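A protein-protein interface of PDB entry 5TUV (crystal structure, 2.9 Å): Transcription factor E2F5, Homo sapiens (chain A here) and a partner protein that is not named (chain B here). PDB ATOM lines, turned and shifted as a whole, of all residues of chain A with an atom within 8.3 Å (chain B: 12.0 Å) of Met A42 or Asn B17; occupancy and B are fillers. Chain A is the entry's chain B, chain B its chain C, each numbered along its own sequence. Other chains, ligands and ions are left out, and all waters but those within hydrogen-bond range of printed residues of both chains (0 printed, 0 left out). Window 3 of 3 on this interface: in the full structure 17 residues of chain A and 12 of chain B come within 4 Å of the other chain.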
ATOM      1  N   GLN A  35     -28.151  -0.553  -6.281  1.00  0.00           N
ATOM      2  CA  GLN A  35     -28.786  -1.752  -5.743  1.00  0.00           C
ATOM      3  C   GLN A  35     -29.581  -2.452  -6.838  1.00  0.00           C
ATOM      4  O   GLN A  35     -29.551  -3.678  -6.951  1.00  0.00           O
ATOM      5  CB  GLN A  35     -29.701  -1.413  -4.563  1.00  0.00           C
ATOM      6  CG  GLN A  35     -28.985  -1.176  -3.249  1.00  0.00           C
ATOM      7  CD  GLN A  35     -29.948  -0.880  -2.121  1.00  0.00           C
ATOM      8  OE1 GLN A  35     -31.025  -0.328  -2.341  1.00  0.00           O
ATOM      9  NE2 GLN A  35     -29.569  -1.254  -0.905  1.00  0.00           N
ATOM     10  N   GLN A  36     -30.291  -1.657  -7.637  1.00  0.00           N
ATOM     11  CA  GLN A  36     -31.086  -2.168  -8.751  1.00  0.00           C
ATOM     12  C   GLN A  36     -30.213  -2.877  -9.767  1.00  0.00           C
ATOM     13  O   GLN A  36     -30.588  -3.919 -10.304  1.00  0.00           O
ATOM     14  CB  GLN A  36     -31.839  -1.046  -9.457  1.00  0.00           C
ATOM     15  CG  GLN A  36     -32.778  -1.546 -10.550  1.00  0.00           C
ATOM     16  CD  GLN A  36     -33.913  -2.384 -10.011  1.00  0.00           C
ATOM     17  OE1 GLN A  36     -34.604  -1.981  -9.075  1.00  0.00           O
ATOM     18  NE2 GLN A  36     -34.111  -3.559 -10.597  1.00  0.00           N
ATOM     19  N   SER A  37     -29.044  -2.307 -10.031  1.00  0.00           N
ATOM     20  CA  SER A  37     -28.138  -2.876 -11.015  1.00  0.00           C
ATOM     21  C   SER A  37     -27.499  -4.141 -10.464  1.00  0.00           C
ATOM     22  O   SER A  37     -27.031  -4.988 -11.220  1.00  0.00           O
ATOM     23  CB  SER A  37     -27.064  -1.862 -11.415  1.00  0.00           C
ATOM     24  OG  SER A  37     -25.959  -1.911 -10.530  1.00  0.00           O
ATOM     25  N   ILE A  38     -27.495  -4.268  -9.142  1.00  0.00           N
ATOM     26  CA  ILE A  38     -26.958  -5.457  -8.494  1.00  0.00           C
ATOM     27  C   ILE A  38     -27.997  -6.572  -8.574  1.00  0.00           C
ATOM     28  O   ILE A  38     -27.660  -7.744  -8.738  1.00  0.00           O
ATOM     29  CB  ILE A  38     -26.576  -5.182  -7.024  1.00  0.00           C
ATOM     30  CG1 ILE A  38     -25.369  -4.248  -6.957  1.00  0.00           C
ATOM     31  CG2 ILE A  38     -26.258  -6.472  -6.292  1.00  0.00           C
ATOM     32  CD1 ILE A  38     -24.993  -3.838  -5.553  1.00  0.00           C
ATOM     33  N   LYS A  39     -29.268  -6.190  -8.482  1.00  0.00           N
ATOM     34  CA  LYS A  39     -30.367  -7.143  -8.577  1.00  0.00           C
ATOM     35  C   LYS A  39     -30.495  -7.717  -9.986  1.00  0.00           C
ATOM     36  O   LYS A  39     -30.877  -8.874 -10.160  1.00  0.00           O
ATOM     37  CB  LYS A  39     -31.684  -6.485  -8.160  1.00  0.00           C
ATOM     38  N   ASN A  40     -30.170  -6.906 -10.989  1.00  0.00           N
ATOM     39  CA  ASN A  40     -30.286  -7.331 -12.380  1.00  0.00           C
ATOM     40  C   ASN A  40     -29.194  -8.317 -12.779  1.00  0.00           C
ATOM     41  O   ASN A  40     -29.403  -9.179 -13.632  1.00  0.00           O
ATOM     42  CB  ASN A  40     -30.244  -6.117 -13.311  1.00  0.00           C
ATOM     43  CG  ASN A  40     -31.510  -5.287 -13.246  1.00  0.00           C
ATOM     44  OD1 ASN A  40     -32.331  -5.454 -12.345  1.00  0.00           O
ATOM     45  ND2 ASN A  40     -31.672  -4.383 -14.204  1.00  0.00           N
ATOM     46  N   VAL A  41     -28.030  -8.183 -12.156  1.00  0.00           N
ATOM     47  CA  VAL A  41     -26.898  -9.060 -12.436  1.00  0.00           C
ATOM     48  C   VAL A  41     -27.072 -10.455 -11.836  1.00  0.00           C
ATOM     49  O   VAL A  41     -26.806 -11.461 -12.497  1.00  0.00           O
ATOM     50  CB  VAL A  41     -25.576  -8.450 -11.917  1.00  0.00           C
ATOM     51  CG1 VAL A  41     -24.434  -9.447 -12.047  1.00  0.00           C
ATOM     52  CG2 VAL A  41     -25.251  -7.171 -12.672  1.00  0.00           C
ATOM     53  N   MET A  42     -27.541 -10.518 -10.593  1.00  0.00           N
ATOM     54  CA  MET A  42     -27.634 -11.793  -9.893  1.00  0.00           C
ATOM     55  C   MET A  42     -28.881 -12.592 -10.271  1.00  0.00           C
ATOM     56  O   MET A  42     -29.045 -13.734  -9.829  1.00  0.00           O
ATOM     57  CB  MET A  42     -27.605 -11.560  -8.381  1.00  0.00           C
ATOM     58  CG  MET A  42     -26.301 -10.956  -7.878  1.00  0.00           C
ATOM     59  SD  MET A  42     -26.173 -10.962  -6.078  1.00  0.00           S
ATOM     60  CE  MET A  42     -27.532  -9.882  -5.639  1.00  0.00           C
ATOM     61  N   ASP A  43     -29.754 -12.001 -11.087  1.00  0.00           N
ATOM     62  CA  ASP A  43     -30.785 -12.787 -11.763  1.00  0.00           C
ATOM     63  C   ASP A  43     -30.661 -12.607 -13.272  1.00  0.00           C
ATOM     64  O   ASP A  43     -31.534 -12.058 -13.945  1.00  0.00           O
ATOM     65  CB  ASP A  43     -32.202 -12.441 -11.286  1.00  0.00           C
ATOM     66  CG  ASP A  43     -33.281 -13.272 -11.998  1.00  0.00           C
ATOM     67  OD1 ASP A  43     -33.553 -14.401 -11.537  1.00  0.00           O
ATOM     68  OD2 ASP A  43     -33.879 -12.802 -12.990  1.00  0.00           O
ATOM     69  N   ASP A  44     -29.515 -13.030 -13.781  1.00  0.00           N
ATOM     70  CA  ASP A  44     -29.422 -13.450 -15.158  1.00  0.00           C
ATOM     71  C   ASP A  44     -29.516 -14.951 -14.916  1.00  0.00           C
ATOM     72  O   ASP A  44     -29.261 -15.397 -13.792  1.00  0.00           O
ATOM     73  CB  ASP A  44     -28.114 -13.008 -15.832  1.00  0.00           C
ATOM     74  CG  ASP A  44     -28.075 -13.335 -17.316  1.00  0.00           C
ATOM     75  OD1 ASP A  44     -29.046 -13.937 -17.824  1.00  0.00           O
ATOM     76  OD2 ASP A  44     -27.069 -12.994 -17.973  1.00  0.00           O
ATOM     77  N   SER A  45     -29.866 -15.735 -15.928  1.00  0.00           N
ATOM     78  CA  SER A  45     -30.012 -17.162 -15.690  1.00  0.00           C
ATOM     79  C   SER A  45     -28.665 -17.824 -15.899  1.00  0.00           C
ATOM     80  O   SER A  45     -28.417 -18.924 -15.388  1.00  0.00           O
ATOM     81  CB  SER A  45     -31.067 -17.790 -16.596  1.00  0.00           C
ATOM     82  OG  SER A  45     -30.853 -17.418 -17.953  1.00  0.00           O
ATOM     83  N   ILE A  46     -27.798 -17.160 -16.661  1.00  0.00           N
ATOM     84  CA  ILE A  46     -26.430 -17.622 -16.828  1.00  0.00           C
ATOM     85  C   ILE A  46     -25.616 -17.309 -15.569  1.00  0.00           C
ATOM     86  O   ILE A  46     -24.796 -18.120 -15.135  1.00  0.00           O
ATOM     87  CB  ILE A  46     -25.754 -16.969 -18.047  1.00  0.00           C
ATOM     88  CG1 ILE A  46     -26.575 -17.172 -19.330  1.00  0.00           C
ATOM     89  CG2 ILE A  46     -24.332 -17.498 -18.221  1.00  0.00           C
ATOM     90  CD1 ILE A  46     -26.187 -16.226 -20.440  1.00  0.00           C
ATOM     91  N   ASN A  47     -25.835 -16.128 -14.994  1.00  0.00           N
ATOM     92  CA  ASN A  47     -25.091 -15.716 -13.808  1.00  0.00           C
ATOM     93  C   ASN A  47     -25.477 -16.523 -12.574  1.00  0.00           C
ATOM     94  O   ASN A  47     -24.625 -16.859 -11.750  1.00  0.00           O
ATOM     95  CB  ASN A  47     -25.290 -14.223 -13.539  1.00  0.00           C
ATOM     96  CG  ASN A  47     -24.560 -13.346 -14.541  1.00  0.00           C
ATOM     97  OD1 ASN A  47     -23.635 -13.795 -15.218  1.00  0.00           O
ATOM     98  ND2 ASN A  47     -24.972 -12.086 -14.638  1.00  0.00           N
ATOM     99  N   ASN A  48     -26.765 -16.832 -12.454  1.00  0.00           N
ATOM    100  CA  ASN A  48     -27.262 -17.647 -11.354  1.00  0.00           C
ATOM    101  C   ASN A  48     -26.687 -19.059 -11.406  1.00  0.00           C
ATOM    102  O   ASN A  48     -26.532 -19.720 -10.379  1.00  0.00           O
ATOM    103  CB  ASN A  48     -28.790 -17.702 -11.384  1.00  0.00           C
ATOM    104  CG  ASN A  48     -29.368 -18.500 -10.233  1.00  0.00           C
ATOM    105  OD1 ASN A  48     -28.896 -18.407  -9.101  1.00  0.00           O
ATOM    106  ND2 ASN A  48     -30.395 -19.293 -10.517  1.00  0.00           N
ATOM    107  N   ARG A  49     -26.375 -19.508 -12.616  1.00  0.00           N
ATOM    108  CA  ARG A  49     -25.800 -20.827 -12.853  1.00  0.00           C
ATOM    109  C   ARG A  49     -24.401 -20.975 -12.244  1.00  0.00           C
ATOM    110  O   ARG A  49     -23.970 -22.082 -11.923  1.00  0.00           O
ATOM    111  CB  ARG A  49     -25.760 -21.099 -14.362  1.00  0.00           C
ATOM    112  CG  ARG A  49     -25.127 -22.414 -14.776  1.00  0.00           C
ATOM    113  CD  ARG A  49     -25.770 -23.597 -14.074  1.00  0.00           C
ATOM    114  NE  ARG A  49     -25.168 -24.860 -14.490  1.00  0.00           N
ATOM    115  CZ  ARG A  49     -23.990 -25.302 -14.062  1.00  0.00           C
ATOM    116  NH1 ARG A  49     -23.281 -24.586 -13.200  1.00  0.00           N
ATOM    117  NH2 ARG A  49     -23.519 -26.463 -14.496  1.00  0.00           N
ATOM    118  N   SER A  51     -23.244 -18.718  -9.636  1.00  0.00           N
ATOM    119  CA  SER A  51     -23.187 -17.981  -8.380  1.00  0.00           C
ATOM    120  C   SER A  51     -23.079 -18.934  -7.191  1.00  0.00           C
ATOM    121  O   SER A  51     -24.025 -19.076  -6.418  1.00  0.00           O
ATOM    122  CB  SER A  51     -24.414 -17.079  -8.228  1.00  0.00           C
ATOM    123  OG  SER A  51     -25.573 -17.834  -7.929  1.00  0.00           O
ATOM    124  N   ALA A  72     -30.627 -20.425   1.710  1.00  0.00           N
ATOM    125  CA  ALA A  72     -32.054 -20.160   1.693  1.00  0.00           C
ATOM    126  C   ALA A  72     -32.338 -19.122   0.609  1.00  0.00           C
ATOM    127  O   ALA A  72     -31.443 -18.368   0.228  1.00  0.00           O
ATOM    128  CB  ALA A  72     -32.528 -19.678   3.052  1.00  0.00           C
ATOM    129  N   PRO A  73     -33.577 -19.089   0.095  1.00  0.00           N
ATOM    130  CA  PRO A  73     -33.927 -18.074  -0.904  1.00  0.00           C
ATOM    131  C   PRO A  73     -33.846 -16.649  -0.366  1.00  0.00           C
ATOM    132  O   PRO A  73     -33.734 -16.446   0.842  1.00  0.00           O
ATOM    133  CB  PRO A  73     -35.375 -18.422  -1.272  1.00  0.00           C
ATOM    134  CG  PRO A  73     -35.872 -19.281  -0.159  1.00  0.00           C
ATOM    135  CD  PRO A  73     -34.683 -20.031   0.337  1.00  0.00           C
ATOM    136  N   SER A  74     -33.893 -15.673  -1.268  1.00  0.00           N
ATOM    137  CA  SER A  74     -33.781 -14.272  -0.886  1.00  0.00           C
ATOM    138  C   SER A  74     -35.003 -13.842  -0.082  1.00  0.00           C
ATOM    139  O   SER A  74     -36.104 -14.352  -0.288  1.00  0.00           O
ATOM    140  CB  SER A  74     -33.617 -13.382  -2.121  1.00  0.00           C
ATOM    141  OG  SER A  74     -32.509 -13.795  -2.901  1.00  0.00           O
ATOM    142  N   GLY A  75     -34.801 -12.904   0.836  1.00  0.00           N
ATOM    143  CA  GLY A  75     -35.873 -12.423   1.686  1.00  0.00           C
ATOM    144  C   GLY A  75     -36.123 -13.323   2.878  1.00  0.00           C
ATOM    145  O   GLY A  75     -37.070 -13.116   3.636  1.00  0.00           O
ATOM    146  N   THR A  76     -35.269 -14.328   3.046  1.00  0.00           N
ATOM    147  CA  THR A  76     -35.366 -15.226   4.189  1.00  0.00           C
ATOM    148  C   THR A  76     -34.946 -14.455   5.432  1.00  0.00           C
ATOM    149  O   THR A  76     -33.885 -13.832   5.449  1.00  0.00           O
ATOM    150  CB  THR A  76     -34.487 -16.477   4.019  1.00  0.00           C
ATOM    151  OG1 THR A  76     -34.837 -17.150   2.803  1.00  0.00           O
ATOM    152  CG2 THR A  76     -34.677 -17.429   5.189  1.00  0.00           C
ATOM    153  N   LEU B  13     -32.372  -8.891  13.849  1.00  0.00           N
ATOM    154  CA  LEU B  13     -32.860  -9.491  12.612  1.00  0.00           C
ATOM    155  C   LEU B  13     -31.829  -9.418  11.490  1.00  0.00           C
ATOM    156  O   LEU B  13     -31.070  -8.455  11.389  1.00  0.00           O
ATOM    157  CB  LEU B  13     -34.156  -8.810  12.157  1.00  0.00           C
ATOM    158  CG  LEU B  13     -35.386  -8.859  13.072  1.00  0.00           C
ATOM    159  CD1 LEU B  13     -35.525 -10.224  13.728  1.00  0.00           C
ATOM    160  CD2 LEU B  13     -35.366  -7.746  14.116  1.00  0.00           C
ATOM    161  N   TYR B  14     -31.812 -10.446  10.648  1.00  0.00           N
ATOM    162  CA  TYR B  14     -30.998 -10.440   9.439  1.00  0.00           C
ATOM    163  C   TYR B  14     -31.782 -11.005   8.260  1.00  0.00           C
ATOM    164  O   TYR B  14     -32.552 -11.954   8.412  1.00  0.00           O
ATOM    165  CB  TYR B  14     -29.707 -11.237   9.638  1.00  0.00           C
ATOM    166  CG  TYR B  14     -28.955 -11.468   8.348  1.00  0.00           C
ATOM    167  CD1 TYR B  14     -28.198 -10.458   7.773  1.00  0.00           C
ATOM    168  CD2 TYR B  14     -29.017 -12.694   7.695  1.00  0.00           C
ATOM    169  CE1 TYR B  14     -27.519 -10.661   6.589  1.00  0.00           C
ATOM    170  CE2 TYR B  14     -28.342 -12.906   6.510  1.00  0.00           C
ATOM    171  CZ  TYR B  14     -27.593 -11.887   5.963  1.00  0.00           C
ATOM    172  OH  TYR B  14     -26.921 -12.097   4.783  1.00  0.00           O
ATOM    173  N   LYS B  15     -31.580 -10.421   7.084  1.00  0.00           N
ATOM    174  CA  LYS B  15     -32.277 -10.860   5.881  1.00  0.00           C
ATOM    175  C   LYS B  15     -31.299 -11.342   4.814  1.00  0.00           C
ATOM    176  O   LYS B  15     -30.339 -10.648   4.479  1.00  0.00           O
ATOM    177  CB  LYS B  15     -33.144  -9.728   5.325  1.00  0.00           C
ATOM    178  CG  LYS B  15     -34.008 -10.129   4.142  1.00  0.00           C
ATOM    179  CD  LYS B  15     -34.867  -8.967   3.673  1.00  0.00           C
ATOM    180  CE  LYS B  15     -35.686  -8.390   4.818  1.00  0.00           C
ATOM    181  NZ  LYS B  15     -36.535  -9.424   5.472  1.00  0.00           N
ATOM    182  N   PHE B  16     -31.550 -12.537   4.288  1.00  0.00           N
ATOM    183  CA  PHE B  16     -30.721 -13.104   3.231  1.00  0.00           C
ATOM    184  C   PHE B  16     -30.795 -12.255   1.966  1.00  0.00           C
ATOM    185  O   PHE B  16     -31.877 -12.048   1.415  1.00  0.00           O
ATOM    186  CB  PHE B  16     -31.150 -14.541   2.919  1.00  0.00           C
ATOM    187  CG  PHE B  16     -30.709 -15.548   3.946  1.00  0.00           C
ATOM    188  CD1 PHE B  16     -31.256 -15.551   5.219  1.00  0.00           C
ATOM    189  CD2 PHE B  16     -29.755 -16.501   3.632  1.00  0.00           C
ATOM    190  CE1 PHE B  16     -30.854 -16.479   6.161  1.00  0.00           C
ATOM    191  CE2 PHE B  16     -29.348 -17.431   4.568  1.00  0.00           C
ATOM    192  CZ  PHE B  16     -29.899 -17.420   5.835  1.00  0.00           C
ATOM    193  N   ASN B  17     -29.638 -11.769   1.521  1.00  0.00           N
ATOM    194  CA  ASN B  17     -29.539 -10.944   0.319  1.00  0.00           C
ATOM    195  C   ASN B  17     -30.453  -9.722   0.397  1.00  0.00           C
ATOM    196  O   ASN B  17     -31.219  -9.443  -0.525  1.00  0.00           O
ATOM    197  CB  ASN B  17     -29.864 -11.780  -0.926  1.00  0.00           C
ATOM    198  CG  ASN B  17     -29.484 -11.082  -2.217  1.00  0.00           C
ATOM    199  OD1 ASN B  17     -28.535 -10.298  -2.258  1.00  0.00           O
ATOM    200  ND2 ASN B  17     -30.224 -11.365  -3.282  1.00  0.00           N
ATOM    201  N   GLY B  18     -30.374  -9.001   1.510  1.00  0.00           N
ATOM    202  CA  GLY B  18     -31.207  -7.830   1.712  1.00  0.00           C
ATOM    203  C   GLY B  18     -30.949  -7.135   3.034  1.00  0.00           C
ATOM    204  O   GLY B  18     -31.733  -6.288   3.465  1.00  0.00           O
ATOM    205  N   SER B  19     -29.846  -7.494   3.682  1.00  0.00           N
ATOM    206  CA  SER B  19     -29.471  -6.886   4.952  1.00  0.00           C
ATOM    207  C   SER B  19     -27.968  -6.640   5.010  1.00  0.00           C
ATOM    208  O   SER B  19     -27.180  -7.505   4.622  1.00  0.00           O
ATOM    209  CB  SER B  19     -29.909  -7.769   6.122  1.00  0.00           C
ATOM    210  OG  SER B  19     -29.650  -7.139   7.364  1.00  0.00           O
ATOM    211  N   PRO B  20     -27.566  -5.453   5.490  1.00  0.00           N
ATOM    212  CA  PRO B  20     -26.154  -5.070   5.609  1.00  0.00           C
ATOM    213  C   PRO B  20     -25.353  -6.039   6.476  1.00  0.00           C
ATOM    214  O   PRO B  20     -25.916  -6.680   7.361  1.00  0.00           O
ATOM    215  CB  PRO B  20     -26.220  -3.685   6.264  1.00  0.00           C
ATOM    216  CG  PRO B  20     -27.573  -3.168   5.915  1.00  0.00           C
ATOM    217  CD  PRO B  20     -28.468  -4.369   5.913  1.00  0.00           C
ATOM    218  N   SER B  21     -24.052  -6.139   6.220  1.00  0.00           N
ATOM    219  CA  SER B  21     -23.182  -7.021   6.992  1.00  0.00           C
ATOM    220  C   SER B  21     -22.934  -6.456   8.386  1.00  0.00           C
ATOM    221  O   SER B  21     -22.421  -7.144   9.269  1.00  0.00           O
ATOM    222  CB  SER B  21     -21.855  -7.241   6.266  1.00  0.00           C
ATOM    223  OG  SER B  21     -22.002  -8.177   5.213  1.00  0.00           O
ATOM    224  N   LYS B  22     -23.301  -5.192   8.570  1.00  0.00           N
ATOM    225  CA  LYS B  22     -23.215  -4.537   9.867  1.00  0.00           C
ATOM    226  C   LYS B  22     -24.200  -5.181  10.842  1.00  0.00           C
ATOM    227  O   LYS B  22     -24.004  -5.149  12.058  1.00  0.00           O
ATOM    228  CB  LYS B  22     -23.493  -3.040   9.716  1.00  0.00           C
ATOM    229  CG  LYS B  22     -23.510  -2.242  11.012  1.00  0.00           C
ATOM    230  CD  LYS B  22     -24.142  -0.867  10.810  1.00  0.00           C
ATOM    231  CE  LYS B  22     -24.101  -0.431   9.349  1.00  0.00           C
ATOM    232  NZ  LYS B  22     -25.015   0.710   9.072  1.00  0.00           N
ATOM    233  N   SER B  23     -25.254  -5.775  10.292  1.00  0.00           N
ATOM    234  CA  SER B  23     -26.268  -6.453  11.092  1.00  0.00           C
ATOM    235  C   SER B  23     -25.707  -7.698  11.771  1.00  0.00           C
ATOM    236  O   SER B  23     -25.955  -7.936  12.953  1.00  0.00           O
ATOM    237  CB  SER B  23     -27.469  -6.829  10.221  1.00  0.00           C
ATOM    238  OG  SER B  23     -28.015  -5.689   9.585  1.00  0.00           O
ATOM    239  N   LEU B  24     -24.952  -8.492  11.017  1.00  0.00           N
ATOM    240  CA  LEU B  24     -24.381  -9.727  11.543  1.00  0.00           C
ATOM    241  C   LEU B  24     -23.266  -9.454  12.547  1.00  0.00           C
ATOM    242  O   LEU B  24     -23.030 -10.252  13.454  1.00  0.00           O
ATOM    243  CB  LEU B  24     -23.855 -10.602  10.404  1.00  0.00           C
ATOM    244  CG  LEU B  24     -24.921 -11.282   9.542  1.00  0.00           C
ATOM    245  CD1 LEU B  24     -24.273 -12.199   8.518  1.00  0.00           C
ATOM    246  CD2 LEU B  24     -25.904 -12.051  10.412  1.00  0.00           C
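OG of Ser A74 sits at hydrogen-bond distance from ND2 of Asn B17 (3.4 Å).
N of Gly A75 sits at hydrogen-bond distance from O of Phe B16 (3.1 Å).
The backbone carbonyl oxygen (O) of Thr A76 lies within hydrogen-bond range of the backbone NH (N) of Phe B16, 2.9 Å away.
Met A42 touches Asn B17.
Phe B16 touches Pro A73.
CA of Ser A74 touches O of Phe B16 (3.7 Å).
Gly A75 touches Lys B15 (CA to CG, 3.8 Å).
Tyr B14 touches Thr A76.
CA of Lys B15 touches O of Thr A76 (3.4 Å).
Of chain B, only Asn B17 (3.6 Å) comes within 4 Å of Met A42.
Of chain A, only Met A42 (3.6 Å) and Ser A74 (3.4 Å) come within 4 Å of Asn B17.
Ile A38 touches none of the printed residues of chain B.
No residue of chain B comes within 4 Å of Lys A39.
No residue of chain B comes within 4 Å of Val A41.
Asp A43 touches none of the printed residues of chain B.
Of chain B, only Phe B16 (3.7 Å) and Asn B17 (3.4 Å) come within 4 Å of Ser A74.
Of the printed residues of chain B, Pro A73 touches Phe B16.
Printed residues of chain A within 4 Å of Tyr B14: Thr A76 (3.8 Å).
Of the printed residues of chain A, Lys B15 touches Gly A75 and Thr A76.
Ala A72 touches none of the printed residues of chain B.
Leu B13 touches none of the printed residues of chain A.
The nearest residue of chain B that does not touch Met A42 is Gly B18 (7.7 Å).
Of the 12 printed residues of chain B, 4 touch a printed residue of chain A.
Hydrophobic or aromatic side chains of chain B that line the printed part of chain A: Phe B16.
Among the printed residues, no Asp or Glu carboxylate lies within 4 Å of a Lys or Arg side-chain nitrogen of the other chain.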
